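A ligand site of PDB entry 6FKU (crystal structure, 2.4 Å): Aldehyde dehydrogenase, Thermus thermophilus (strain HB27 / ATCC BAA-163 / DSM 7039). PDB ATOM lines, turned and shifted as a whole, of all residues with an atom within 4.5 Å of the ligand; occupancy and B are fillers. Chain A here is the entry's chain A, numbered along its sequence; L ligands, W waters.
An oxygen (O15) of the ligand sits close to the backbone carbonyl oxygen of Gly 219 (3.4 Å).
O11 of the ligand lies close to O of Gly 245 (3.4 Å).
Ile 161 touches the ligand.
CB of Ala 163 touches O10 of the ligand, 3.7 Å away.
ND2 of Asn 165 touches C21 of the ligand (3.3 Å).
CA of Gly 220 touches O15 of the ligand (3.5 Å).
Gly 221 touches the ligand (CA to C10, 3.4 Å).
Lys 222 touches the ligand.
C of Gly 226 touches C9 of the ligand (3.3 Å).
Gln 227 touches the ligand (N to C9, 3.4 Å).
CG2 of Val 230 touches C9 of the ligand (3.98 Å).
Phe 243 touches the ligand (CE1 to O4, 3.4 Å).
CG2 of Thr 244 touches C17 of the ligand, 3.4 Å away.
Val 249 touches the ligand.
Trp 252 touches the ligand (CZ3 to N4, 3.5 Å).
CA of Gly 269 touches O13 of the ligand, at 3.1 Å.
Cys 301 touches the ligand.
CE1 of Phe 349 touches O8 of the ligand, 3.1 Å away.
Phe 412 touches the ligand (CZ to C14, 3.4 Å).
Phe 477 touches the ligand (CE1 to O14, 3.5 Å).
Hydrophobic or aromatic side chains that line the ligand: Ile 161, Ala 163, Val 230, Phe 243, Val 249, Trp 252, Phe 349, Phe 412 and Phe 477.
The nearest printed residue that does not touch the ligand is Pro 189 (4.1 Å).
O12 of the ligand is in hydrogen-bond range of OE1 of Glu 410 (2.6 Å).
The guanidinium group (NH1) of Arg 348 is in salt-bridge range of an oxygen (O8) of the ligand.
The backbone NH of Glu 191 lies close to an oxygen (O15) of the ligand, 3.2 Å away.
OE1 of Glu 191 lies close to O15 of the ligand.
The backbone carbonyl oxygen (O) of Thr 162 lies within hydrogen-bond range of an oxygen (O5) of the ligand (2.7 Å).
The backbone NH (N) of Ser 246 is in hydrogen-bond range of an oxygen (O2) of the ligand (2.9 Å).
An oxygen (O2) of the ligand is in hydrogen-bond range of the side-chain hydroxyl of Ser 246 (2.9 Å).
O of Leu 268 sits at hydrogen-bond distance from N7 of the ligand, at 3.0 Å.
The side-chain amino group of Lys 188 is in salt-bridge range of an oxygen (O15) of the ligand (3.2 Å).
O17 of the ligand is in hydrogen-bond range of OG of Ser 190, 3.1 Å away.
The backbone carbonyl oxygen of Glu 267 lies close to a nitrogen (N7) of the ligand, at 3.5 Å.
The side-chain carboxylate (OE2) of Glu 410 is in hydrogen-bond range of the backbone NH (N) of Gly 270.
N of Thr 162 lies within hydrogen-bond range of O of Lys 188 (3.5 Å).
The backbone NH of Ser 190 lies within hydrogen-bond range of the backbone carbonyl oxygen of Thr 162.
The backbone carbonyl oxygen (O) of Glu 267 lies within hydrogen-bond range of the backbone NH (N) of Gly 245 (3.1 Å).
N of Glu 267 is in hydrogen-bond range of O of Phe 243, 3.0 Å away.
The backbone NH (N) of Thr 244 sits at hydrogen-bond distance from the backbone carbonyl oxygen (O) of Ile 161 (3.1 Å).
The backbone NH (N) of Gly 226 is in hydrogen-bond range of the backbone carbonyl oxygen (O) of Gly 220, 2.9 Å away.
The backbone carbonyl oxygen of Gly 221 is in hydrogen-bond range of the backbone NH of Gln 227 (3.0 Å).
Water W2 bridges OG1 of Thr 244 (2.4 Å) and O14 of the ligand (2.7 Å).
Water W1 bridges NH2 of Arg 348 (2.6 Å) and O17 of the ligand (2.9 Å).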
ATOM      1  N   ILE A 161      15.793 -22.091  19.509  1.00  0.00           N
ATOM      2  CA  ILE A 161      16.697 -23.230  19.401  1.00  0.00           C
ATOM      3  C   ILE A 161      16.130 -24.365  20.258  1.00  0.00           C
ATOM      4  O   ILE A 161      15.843 -24.151  21.417  1.00  0.00           O
ATOM      5  CB  ILE A 161      18.129 -22.847  19.834  1.00  0.00           C
ATOM      6  CG1 ILE A 161      18.734 -21.762  18.939  1.00  0.00           C
ATOM      7  CG2 ILE A 161      19.031 -24.083  19.908  1.00  0.00           C
ATOM      8  CD1 ILE A 161      20.134 -21.321  19.348  1.00  0.00           C
ATOM      9  N   THR A 162      16.021 -25.563  19.688  1.00  0.00           N
ATOM     10  CA  THR A 162      15.360 -26.674  20.374  1.00  0.00           C
ATOM     11  C   THR A 162      16.194 -27.966  20.320  1.00  0.00           C
ATOM     12  O   THR A 162      16.930 -28.267  19.360  1.00  0.00           O
ATOM     13  CB  THR A 162      13.976 -26.937  19.772  1.00  0.00           C
ATOM     14  OG1 THR A 162      14.126 -27.162  18.363  1.00  0.00           O
ATOM     15  CG2 THR A 162      13.031 -25.779  19.997  1.00  0.00           C
ATOM     16  N   ALA A 163      16.018 -28.735  21.382  1.00  0.00           N
ATOM     17  CA  ALA A 163      16.504 -30.092  21.486  1.00  0.00           C
ATOM     18  C   ALA A 163      15.661 -30.993  20.593  1.00  0.00           C
ATOM     19  O   ALA A 163      14.688 -30.542  20.019  1.00  0.00           O
ATOM     20  CB  ALA A 163      16.440 -30.521  22.931  1.00  0.00           C
ATOM     21  N   ASN A 165      14.757 -34.396  21.665  1.00  0.00           N
ATOM     22  CA  ASN A 165      14.114 -35.487  22.412  1.00  0.00           C
ATOM     23  C   ASN A 165      12.583 -35.398  22.311  1.00  0.00           C
ATOM     24  O   ASN A 165      11.899 -36.401  22.468  1.00  0.00           O
ATOM     25  CB  ASN A 165      14.588 -35.540  23.873  1.00  0.00           C
ATOM     26  CG  ASN A 165      14.357 -34.276  24.671  1.00  0.00           C
ATOM     27  OD1 ASN A 165      14.185 -33.202  24.100  1.00  0.00           O
ATOM     28  ND2 ASN A 165      14.366 -34.401  25.994  1.00  0.00           N
ATOM     29  N   VAL A 170       7.858 -30.038  21.574  1.00  0.00           N
ATOM     30  CA  VAL A 170       8.559 -28.972  22.269  1.00  0.00           C
ATOM     31  C   VAL A 170       8.718 -27.762  21.336  1.00  0.00           C
ATOM     32  O   VAL A 170       8.525 -26.643  21.758  1.00  0.00           O
ATOM     33  CB  VAL A 170       9.902 -29.474  22.847  1.00  0.00           C
ATOM     34  CG1 VAL A 170      10.992 -28.413  22.841  1.00  0.00           C
ATOM     35  CG2 VAL A 170       9.707 -30.015  24.255  1.00  0.00           C
ATOM     36  N   TRP A 173       5.471 -25.763  21.180  1.00  0.00           N
ATOM     37  CA  TRP A 173       5.225 -24.916  22.362  1.00  0.00           C
ATOM     38  C   TRP A 173       5.734 -23.497  22.129  1.00  0.00           C
ATOM     39  O   TRP A 173       5.282 -22.578  22.810  1.00  0.00           O
ATOM     40  CB  TRP A 173       5.873 -25.469  23.634  1.00  0.00           C
ATOM     41  CG  TRP A 173       5.414 -26.823  24.084  1.00  0.00           C
ATOM     42  CD1 TRP A 173       4.343 -27.536  23.622  1.00  0.00           C
ATOM     43  CD2 TRP A 173       6.020 -27.631  25.104  1.00  0.00           C
ATOM     44  NE1 TRP A 173       4.256 -28.734  24.267  1.00  0.00           N
ATOM     45  CE2 TRP A 173       5.264 -28.821  25.195  1.00  0.00           C
ATOM     46  CE3 TRP A 173       7.112 -27.453  25.962  1.00  0.00           C
ATOM     47  CZ2 TRP A 173       5.570 -29.825  26.111  1.00  0.00           C
ATOM     48  CZ3 TRP A 173       7.424 -28.455  26.856  1.00  0.00           C
ATOM     49  CH2 TRP A 173       6.657 -29.623  26.942  1.00  0.00           C
ATOM     50  N   LYS A 188      16.255 -22.855  14.670  1.00  0.00           N
ATOM     51  CA  LYS A 188      17.382 -23.758  14.515  1.00  0.00           C
ATOM     52  C   LYS A 188      17.031 -25.077  15.216  1.00  0.00           C
ATOM     53  O   LYS A 188      17.168 -25.180  16.427  1.00  0.00           O
ATOM     54  CB  LYS A 188      18.647 -23.126  15.114  1.00  0.00           C
ATOM     55  CG  LYS A 188      19.959 -23.611  14.515  1.00  0.00           C
ATOM     56  CD  LYS A 188      20.202 -25.097  14.635  1.00  0.00           C
ATOM     57  CE  LYS A 188      20.548 -25.506  16.057  1.00  0.00           C
ATOM     58  NZ  LYS A 188      20.796 -26.968  16.150  1.00  0.00           N
ATOM     59  N   PRO A 189      16.546 -26.076  14.459  1.00  0.00           N
ATOM     60  CA  PRO A 189      16.168 -27.351  15.079  1.00  0.00           C
ATOM     61  C   PRO A 189      17.392 -28.181  15.487  1.00  0.00           C
ATOM     62  O   PRO A 189      18.483 -27.972  14.962  1.00  0.00           O
ATOM     63  CB  PRO A 189      15.374 -28.143  14.025  1.00  0.00           C
ATOM     64  CG  PRO A 189      15.192 -27.170  12.876  1.00  0.00           C
ATOM     65  CD  PRO A 189      16.287 -26.131  13.021  1.00  0.00           C
ATOM     66  N   SER A 190      17.183 -29.102  16.427  1.00  0.00           N
ATOM     67  CA  SER A 190      18.174 -30.118  16.746  1.00  0.00           C
ATOM     68  C   SER A 190      18.581 -30.868  15.478  1.00  0.00           C
ATOM     69  O   SER A 190      17.732 -31.239  14.654  1.00  0.00           O
ATOM     70  CB  SER A 190      17.652 -31.099  17.773  1.00  0.00           C
ATOM     71  OG  SER A 190      18.501 -32.238  17.856  1.00  0.00           O
ATOM     72  N   GLU A 191      19.878 -31.136  15.367  1.00  0.00           N
ATOM     73  CA  GLU A 191      20.416 -31.954  14.265  1.00  0.00           C
ATOM     74  C   GLU A 191      20.027 -33.432  14.458  1.00  0.00           C
ATOM     75  O   GLU A 191      20.305 -34.245  13.598  1.00  0.00           O
ATOM     76  CB  GLU A 191      21.932 -31.799  14.160  1.00  0.00           C
ATOM     77  CG  GLU A 191      22.720 -32.401  15.306  1.00  0.00           C
ATOM     78  CD  GLU A 191      24.203 -32.058  15.262  1.00  0.00           C
ATOM     79  OE1 GLU A 191      24.632 -31.119  15.981  1.00  0.00           O
ATOM     80  OE2 GLU A 191      24.944 -32.734  14.509  1.00  0.00           O
ATOM     81  N   GLY A 219      21.625 -27.027  11.286  1.00  0.00           N
ATOM     82  CA  GLY A 219      23.028 -27.046  11.639  1.00  0.00           C
ATOM     83  C   GLY A 219      23.219 -27.549  13.052  1.00  0.00           C
ATOM     84  O   GLY A 219      22.274 -28.061  13.667  1.00  0.00           O
ATOM     85  N   GLY A 220      24.452 -27.417  13.544  1.00  0.00           N
ATOM     86  CA  GLY A 220      24.819 -27.896  14.866  1.00  0.00           C
ATOM     87  C   GLY A 220      24.569 -26.850  15.935  1.00  0.00           C
ATOM     88  O   GLY A 220      23.789 -25.925  15.738  1.00  0.00           O
ATOM     89  N   GLY A 221      25.229 -27.030  17.068  1.00  0.00           N
ATOM     90  CA  GLY A 221      25.159 -26.113  18.187  1.00  0.00           C
ATOM     91  C   GLY A 221      26.465 -25.369  18.388  1.00  0.00           C
ATOM     92  O   GLY A 221      26.714 -24.371  17.743  1.00  0.00           O
ATOM     93  N   LYS A 222      27.291 -25.832  19.319  1.00  0.00           N
ATOM     94  CA  LYS A 222      28.546 -25.137  19.618  1.00  0.00           C
ATOM     95  C   LYS A 222      29.457 -25.217  18.391  1.00  0.00           C
ATOM     96  O   LYS A 222      29.546 -26.252  17.738  1.00  0.00           O
ATOM     97  CB  LYS A 222      29.228 -25.758  20.839  1.00  0.00           C
ATOM     98  CG  LYS A 222      30.435 -24.962  21.323  1.00  0.00           C
ATOM     99  CD  LYS A 222      30.845 -25.332  22.705  1.00  0.00           C
ATOM    100  CE  LYS A 222      31.782 -24.312  23.324  1.00  0.00           C
ATOM    101  NZ  LYS A 222      32.140 -24.718  24.712  1.00  0.00           N
ATOM    102  N   GLY A 226      23.770 -23.060  15.740  1.00  0.00           N
ATOM    103  CA  GLY A 226      23.219 -22.673  17.034  1.00  0.00           C
ATOM    104  C   GLY A 226      23.992 -21.546  17.669  1.00  0.00           C
ATOM    105  O   GLY A 226      23.431 -20.507  18.010  1.00  0.00           O
ATOM    106  N   GLN A 227      25.289 -21.745  17.861  1.00  0.00           N
ATOM    107  CA  GLN A 227      26.114 -20.723  18.486  1.00  0.00           C
ATOM    108  C   GLN A 227      26.005 -19.412  17.689  1.00  0.00           C
ATOM    109  O   GLN A 227      25.854 -18.342  18.290  1.00  0.00           O
ATOM    110  CB  GLN A 227      27.573 -21.179  18.575  1.00  0.00           C
ATOM    111  CG  GLN A 227      28.493 -20.164  19.250  1.00  0.00           C
ATOM    112  CD  GLN A 227      29.950 -20.509  19.055  1.00  0.00           C
ATOM    113  OE1 GLN A 227      30.369 -21.651  19.200  1.00  0.00           O
ATOM    114  NE2 GLN A 227      30.734 -19.501  18.719  1.00  0.00           N
ATOM    115  N   VAL A 230      22.834 -17.488  18.378  1.00  0.00           N
ATOM    116  CA  VAL A 230      22.826 -16.817  19.690  1.00  0.00           C
ATOM    117  C   VAL A 230      23.620 -15.508  19.589  1.00  0.00           C
ATOM    118  O   VAL A 230      23.194 -14.467  20.096  1.00  0.00           O
ATOM    119  CB  VAL A 230      23.395 -17.735  20.796  1.00  0.00           C
ATOM    120  CG1 VAL A 230      23.589 -17.006  22.111  1.00  0.00           C
ATOM    121  CG2 VAL A 230      22.529 -18.969  21.000  1.00  0.00           C
ATOM    122  N   PHE A 243      14.690 -21.121  24.174  1.00  0.00           N
ATOM    123  CA  PHE A 243      15.651 -22.208  24.154  1.00  0.00           C
ATOM    124  C   PHE A 243      15.145 -23.370  25.013  1.00  0.00           C
ATOM    125  O   PHE A 243      14.638 -23.155  26.121  1.00  0.00           O
ATOM    126  CB  PHE A 243      17.014 -21.756  24.658  1.00  0.00           C
ATOM    127  CG  PHE A 243      18.030 -22.864  24.819  1.00  0.00           C
ATOM    128  CD1 PHE A 243      18.647 -23.426  23.710  1.00  0.00           C
ATOM    129  CD2 PHE A 243      18.370 -23.341  26.075  1.00  0.00           C
ATOM    130  CE1 PHE A 243      19.593 -24.432  23.853  1.00  0.00           C
ATOM    131  CE2 PHE A 243      19.306 -24.356  26.219  1.00  0.00           C
ATOM    132  CZ  PHE A 243      19.914 -24.898  25.115  1.00  0.00           C
ATOM    133  N   THR A 244      15.280 -24.567  24.467  1.00  0.00           N
ATOM    134  CA  THR A 244      15.104 -25.790  25.214  1.00  0.00           C
ATOM    135  C   THR A 244      16.381 -26.629  25.065  1.00  0.00           C
ATOM    136  O   THR A 244      16.784 -26.943  23.944  1.00  0.00           O
ATOM    137  CB  THR A 244      13.870 -26.565  24.740  1.00  0.00           C
ATOM    138  OG1 THR A 244      12.705 -25.857  25.163  1.00  0.00           O
ATOM    139  CG2 THR A 244      13.825 -27.977  25.287  1.00  0.00           C
ATOM    140  N   GLY A 245      17.006 -26.976  26.189  1.00  0.00           N
ATOM    141  CA  GLY A 245      18.258 -27.717  26.156  1.00  0.00           C
ATOM    142  C   GLY A 245      18.945 -27.758  27.514  1.00  0.00           C
ATOM    143  O   GLY A 245      18.294 -27.690  28.550  1.00  0.00           O
ATOM    144  N   SER A 246      20.258 -27.837  27.492  1.00  0.00           N
ATOM    145  CA  SER A 246      21.054 -28.013  28.708  1.00  0.00           C
ATOM    146  C   SER A 246      21.192 -26.693  29.478  1.00  0.00           C
ATOM    147  O   SER A 246      21.177 -25.596  28.903  1.00  0.00           O
ATOM    148  CB  SER A 246      22.407 -28.590  28.375  1.00  0.00           C
ATOM    149  OG  SER A 246      23.151 -27.667  27.586  1.00  0.00           O
ATOM    150  N   VAL A 249      24.318 -24.544  28.384  1.00  0.00           N
ATOM    151  CA  VAL A 249      24.097 -23.694  27.202  1.00  0.00           C
ATOM    152  C   VAL A 249      23.104 -22.572  27.570  1.00  0.00           C
ATOM    153  O   VAL A 249      23.246 -21.441  27.077  1.00  0.00           O
ATOM    154  CB  VAL A 249      23.596 -24.529  26.008  1.00  0.00           C
ATOM    155  CG1 VAL A 249      23.154 -23.648  24.844  1.00  0.00           C
ATOM    156  CG2 VAL A 249      24.644 -25.521  25.534  1.00  0.00           C
ATOM    157  N   TRP A 252      24.623 -19.468  29.102  1.00  0.00           N
ATOM    158  CA  TRP A 252      25.250 -18.605  28.113  1.00  0.00           C
ATOM    159  C   TRP A 252      24.191 -17.841  27.320  1.00  0.00           C
ATOM    160  O   TRP A 252      24.335 -16.626  27.091  1.00  0.00           O
ATOM    161  CB  TRP A 252      26.172 -19.396  27.171  1.00  0.00           C
ATOM    162  CG  TRP A 252      26.768 -18.540  26.105  1.00  0.00           C
ATOM    163  CD1 TRP A 252      27.534 -17.418  26.271  1.00  0.00           C
ATOM    164  CD2 TRP A 252      26.628 -18.711  24.682  1.00  0.00           C
ATOM    165  NE1 TRP A 252      27.891 -16.890  25.052  1.00  0.00           N
ATOM    166  CE2 TRP A 252      27.343 -17.667  24.066  1.00  0.00           C
ATOM    167  CE3 TRP A 252      25.981 -19.656  23.879  1.00  0.00           C
ATOM    168  CZ2 TRP A 252      27.422 -17.533  22.682  1.00  0.00           C
ATOM    169  CZ3 TRP A 252      26.062 -19.533  22.504  1.00  0.00           C
ATOM    170  CH2 TRP A 252      26.775 -18.483  21.920  1.00  0.00           C
ATOM    171  N   GLU A 267      14.115 -23.262  29.036  1.00  0.00           N
ATOM    172  CA  GLU A 267      13.633 -24.524  29.570  1.00  0.00           C
ATOM    173  C   GLU A 267      14.820 -25.484  29.631  1.00  0.00           C
ATOM    174  O   GLU A 267      15.294 -25.968  28.589  1.00  0.00           O
ATOM    175  CB  GLU A 267      12.491 -25.028  28.691  1.00  0.00           C
ATOM    176  CG  GLU A 267      11.314 -24.074  28.595  1.00  0.00           C
ATOM    177  CD  GLU A 267      10.302 -24.204  29.728  1.00  0.00           C
ATOM    178  OE1 GLU A 267      10.557 -24.982  30.662  1.00  0.00           O
ATOM    179  OE2 GLU A 267       9.262 -23.525  29.678  1.00  0.00           O
ATOM    180  N   LEU A 268      15.324 -25.746  30.820  1.00  0.00           N
ATOM    181  CA  LEU A 268      16.637 -26.385  30.955  1.00  0.00           C
ATOM    182  C   LEU A 268      16.478 -27.733  31.646  1.00  0.00           C
ATOM    183  O   LEU A 268      15.398 -28.331  31.601  1.00  0.00           O
ATOM    184  CB  LEU A 268      17.582 -25.435  31.707  1.00  0.00           C
ATOM    185  CG  LEU A 268      17.599 -23.985  31.203  1.00  0.00           C
ATOM    186  CD1 LEU A 268      18.503 -23.106  32.057  1.00  0.00           C
ATOM    187  CD2 LEU A 268      18.027 -23.919  29.744  1.00  0.00           C
ATOM    188  N   GLY A 269      17.534 -28.231  32.274  1.00  0.00           N
ATOM    189  CA  GLY A 269      17.550 -29.612  32.770  1.00  0.00           C
ATOM    190  C   GLY A 269      16.756 -29.816  34.047  1.00  0.00           C
ATOM    191  O   GLY A 269      16.149 -28.895  34.609  1.00  0.00           O
ATOM    192  N   GLY A 270      16.774 -31.061  34.512  1.00  0.00           N
ATOM    193  CA  GLY A 270      16.156 -31.433  35.759  1.00  0.00           C
ATOM    194  C   GLY A 270      16.928 -32.539  36.460  1.00  0.00           C
ATOM    195  O   GLY A 270      17.677 -33.285  35.840  1.00  0.00           O
ATOM    196  N   CYS A 301      13.555 -34.207  29.957  1.00  0.00           N
ATOM    197  CA  CYS A 301      13.869 -33.175  30.970  1.00  0.00           C
ATOM    198  C   CYS A 301      13.268 -33.584  32.332  1.00  0.00           C
ATOM    199  O   CYS A 301      13.864 -33.359  33.381  1.00  0.00           O
ATOM    200  CB  CYS A 301      13.342 -31.809  30.544  1.00  0.00           C
ATOM    201  SG  CYS A 301      11.707 -31.823  29.742  1.00  0.00           S
ATOM    202  N   ARG A 348      26.227 -38.286  22.052  1.00  0.00           N
ATOM    203  CA  ARG A 348      26.518 -37.436  23.227  1.00  0.00           C
ATOM    204  C   ARG A 348      25.834 -38.014  24.477  1.00  0.00           C
ATOM    205  O   ARG A 348      26.480 -38.142  25.538  1.00  0.00           O
ATOM    206  CB  ARG A 348      25.969 -36.014  23.066  1.00  0.00           C
ATOM    207  CG  ARG A 348      26.600 -35.194  21.944  1.00  0.00           C
ATOM    208  CD  ARG A 348      26.030 -33.781  21.943  1.00  0.00           C
ATOM    209  NE  ARG A 348      24.634 -33.755  21.537  1.00  0.00           N
ATOM    210  CZ  ARG A 348      23.646 -33.220  22.254  1.00  0.00           C
ATOM    211  NH1 ARG A 348      23.861 -32.766  23.487  1.00  0.00           N
ATOM    212  NH2 ARG A 348      22.441 -33.137  21.728  1.00  0.00           N
ATOM    213  N   PHE A 349      24.543 -38.306  24.368  1.00  0.00           N
ATOM    214  CA  PHE A 349      23.793 -38.830  25.507  1.00  0.00           C
ATOM    215  C   PHE A 349      24.389 -40.192  25.917  1.00  0.00           C
ATOM    216  O   PHE A 349      24.542 -40.489  27.123  1.00  0.00           O
ATOM    217  CB  PHE A 349      22.298 -38.982  25.211  1.00  0.00           C
ATOM    218  CG  PHE A 349      21.557 -37.721  24.830  1.00  0.00           C
ATOM    219  CD1 PHE A 349      22.019 -36.470  25.186  1.00  0.00           C
ATOM    220  CD2 PHE A 349      20.353 -37.800  24.152  1.00  0.00           C
ATOM    221  CE1 PHE A 349      21.313 -35.321  24.852  1.00  0.00           C
ATOM    222  CE2 PHE A 349      19.644 -36.659  23.806  1.00  0.00           C
ATOM    223  CZ  PHE A 349      20.116 -35.420  24.168  1.00  0.00           C
ATOM    224  N   GLU A 410      22.241 -34.070  36.304  1.00  0.00           N
ATOM    225  CA  GLU A 410      21.346 -34.678  35.327  1.00  0.00           C
ATOM    226  C   GLU A 410      22.130 -35.691  34.476  1.00  0.00           C
ATOM    227  O   GLU A 410      23.210 -35.375  33.994  1.00  0.00           O
ATOM    228  CB  GLU A 410      20.737 -33.602  34.424  1.00  0.00           C
ATOM    229  CG  GLU A 410      19.823 -34.177  33.363  1.00  0.00           C
ATOM    230  CD  GLU A 410      19.121 -33.138  32.509  1.00  0.00           C
ATOM    231  OE1 GLU A 410      19.835 -32.299  31.910  1.00  0.00           O
ATOM    232  OE2 GLU A 410      17.872 -33.156  32.446  1.00  0.00           O
ATOM    233  N   PHE A 412      21.013 -37.950  31.245  1.00  0.00           N
ATOM    234  CA  PHE A 412      20.106 -38.483  30.241  1.00  0.00           C
ATOM    235  C   PHE A 412      20.423 -39.966  30.000  1.00  0.00           C
ATOM    236  O   PHE A 412      21.585 -40.356  29.922  1.00  0.00           O
ATOM    237  CB  PHE A 412      20.217 -37.712  28.924  1.00  0.00           C
ATOM    238  CG  PHE A 412      19.092 -36.750  28.660  1.00  0.00           C
ATOM    239  CD1 PHE A 412      18.531 -36.011  29.692  1.00  0.00           C
ATOM    240  CD2 PHE A 412      18.598 -36.577  27.371  1.00  0.00           C
ATOM    241  CE1 PHE A 412      17.489 -35.134  29.457  1.00  0.00           C
ATOM    242  CE2 PHE A 412      17.544 -35.697  27.128  1.00  0.00           C
ATOM    243  CZ  PHE A 412      16.996 -34.972  28.176  1.00  0.00           C
ATOM    244  N   LEU A 438      12.665 -28.599  38.252  1.00  0.00           N
ATOM    245  CA  LEU A 438      11.752 -28.710  37.143  1.00  0.00           C
ATOM    246  C   LEU A 438      10.501 -29.462  37.605  1.00  0.00           C
ATOM    247  O   LEU A 438       9.559 -28.825  38.067  1.00  0.00           O
ATOM    248  CB  LEU A 438      12.480 -29.388  35.976  1.00  0.00           C
ATOM    249  CG  LEU A 438      11.703 -29.434  34.657  1.00  0.00           C
ATOM    250  CD1 LEU A 438      11.268 -28.046  34.222  1.00  0.00           C
ATOM    251  CD2 LEU A 438      12.524 -30.091  33.565  1.00  0.00           C
ATOM    252  N   PHE A 477       4.375 -24.945  31.929  1.00  0.00           N
ATOM    253  CA  PHE A 477       5.519 -25.856  31.967  1.00  0.00           C
ATOM    254  C   PHE A 477       6.810 -25.049  32.089  1.00  0.00           C
ATOM    255  O   PHE A 477       7.066 -24.153  31.299  1.00  0.00           O
ATOM    256  CB  PHE A 477       5.546 -26.718  30.701  1.00  0.00           C
ATOM    257  CG  PHE A 477       6.510 -27.876  30.752  1.00  0.00           C
ATOM    258  CD1 PHE A 477       7.865 -27.682  30.495  1.00  0.00           C
ATOM    259  CD2 PHE A 477       6.064 -29.157  31.034  1.00  0.00           C
ATOM    260  CE1 PHE A 477       8.747 -28.758  30.528  1.00  0.00           C
ATOM    261  CE2 PHE A 477       6.947 -30.232  31.067  1.00  0.00           C
ATOM    262  CZ  PHE A 477       8.281 -30.026  30.806  1.00  0.00           C
HETATM  263  P1  LIG L   1      21.739 -29.108  24.103  1.00  0.00           P
HETATM  264  O1  LIG L   1      22.937 -30.043  23.832  1.00  0.00           O
HETATM  265  O2  LIG L   1      21.836 -27.886  25.023  1.00  0.00           O
HETATM  266  O3  LIG L   1      21.164 -28.682  22.667  1.00  0.00           O
HETATM  267  C1  LIG L   1      19.844 -28.170  22.502  1.00  0.00           C
HETATM  268  C2  LIG L   1      19.806 -27.338  21.231  1.00  0.00           C
HETATM  269  O4  LIG L   1      20.801 -26.330  21.312  1.00  0.00           O
HETATM  270  C3  LIG L   1      20.135 -28.135  19.996  1.00  0.00           C
HETATM  271  O5  LIG L   1      19.504 -27.505  18.889  1.00  0.00           O
HETATM  272  C4  LIG L   1      21.626 -28.007  19.882  1.00  0.00           C
HETATM  273  O6  LIG L   1      22.111 -28.305  18.588  1.00  0.00           O
HETATM  274  C5  LIG L   1      21.831 -26.572  20.353  1.00  0.00           C
HETATM  275  N1  LIG L   1      23.120 -26.267  21.017  1.00  0.00           N
HETATM  276  C6  LIG L   1      23.974 -27.091  21.672  1.00  0.00           C
HETATM  277  N2  LIG L   1      25.031 -26.386  22.125  1.00  0.00           N
HETATM  278  C7  LIG L   1      24.860 -25.100  21.777  1.00  0.00           C
HETATM  279  C8  LIG L   1      25.588 -23.833  21.956  1.00  0.00           C
HETATM  280  N3  LIG L   1      26.763 -23.799  22.613  1.00  0.00           N
HETATM  281  N4  LIG L   1      25.053 -22.709  21.450  1.00  0.00           N
HETATM  282  C9  LIG L   1      23.879 -22.712  20.787  1.00  0.00           C
HETATM  283  N5  LIG L   1      23.164 -23.833  20.577  1.00  0.00           N
HETATM  284  C10 LIG L   1      23.603 -25.024  21.053  1.00  0.00           C
HETATM  285  O7  LIG L   1      20.509 -30.037  24.656  1.00  0.00           O
HETATM  286  P2  LIG L   1      20.389 -31.599  24.227  1.00  0.00           P
HETATM  287  O8  LIG L   1      21.623 -32.254  24.828  1.00  0.00           O
HETATM  288  O9  LIG L   1      20.243 -31.644  22.702  1.00  0.00           O
HETATM  289  O10 LIG L   1      19.049 -32.030  25.015  1.00  0.00           O
HETATM  290  C11 LIG L   1      19.108 -32.461  26.378  1.00  0.00           C
HETATM  291  C12 LIG L   1      18.882 -31.303  27.346  1.00  0.00           C
HETATM  292  O11 LIG L   1      17.669 -30.623  26.984  1.00  0.00           O
HETATM  293  C13 LIG L   1      18.708 -31.779  28.779  1.00  0.00           C
HETATM  294  O12 LIG L   1      19.454 -30.961  29.682  1.00  0.00           O
HETATM  295  C14 LIG L   1      17.203 -31.637  29.004  1.00  0.00           C
HETATM  296  O13 LIG L   1      16.807 -31.469  30.359  1.00  0.00           O
HETATM  297  C15 LIG L   1      16.849 -30.440  28.132  1.00  0.00           C
HETATM  298  N6  LIG L   1      15.412 -30.418  27.851  1.00  0.00           N
HETATM  299  C16 LIG L   1      14.667 -29.479  28.471  1.00  0.00           C
HETATM  300  C17 LIG L   1      13.284 -29.412  28.267  1.00  0.00           C
HETATM  301  C18 LIG L   1      12.454 -28.363  28.968  1.00  0.00           C
HETATM  302  O14 LIG L   1      11.409 -28.012  28.427  1.00  0.00           O
HETATM  303  N7  LIG L   1      12.847 -27.883  30.162  1.00  0.00           N
HETATM  304  C19 LIG L   1      12.675 -30.342  27.406  1.00  0.00           C
HETATM  305  C20 LIG L   1      13.468 -31.316  26.779  1.00  0.00           C
HETATM  306  C21 LIG L   1      14.854 -31.328  27.022  1.00  0.00           C
HETATM  307  P3  LIG L   1      22.319 -29.881  18.150  1.00  0.00           P
HETATM  308  O15 LIG L   1      22.462 -29.706  16.642  1.00  0.00           O
HETATM  309  O16 LIG L   1      23.551 -30.363  18.894  1.00  0.00           O
HETATM  310  O17 LIG L   1      21.066 -30.672  18.533  1.00  0.00           O
HETATM  311  O   HOH W   1      22.275 -33.261  19.182  1.00  0.00           O
HETATM  312  O   HOH W   2      10.662 -26.328  26.408  1.00  0.00           O
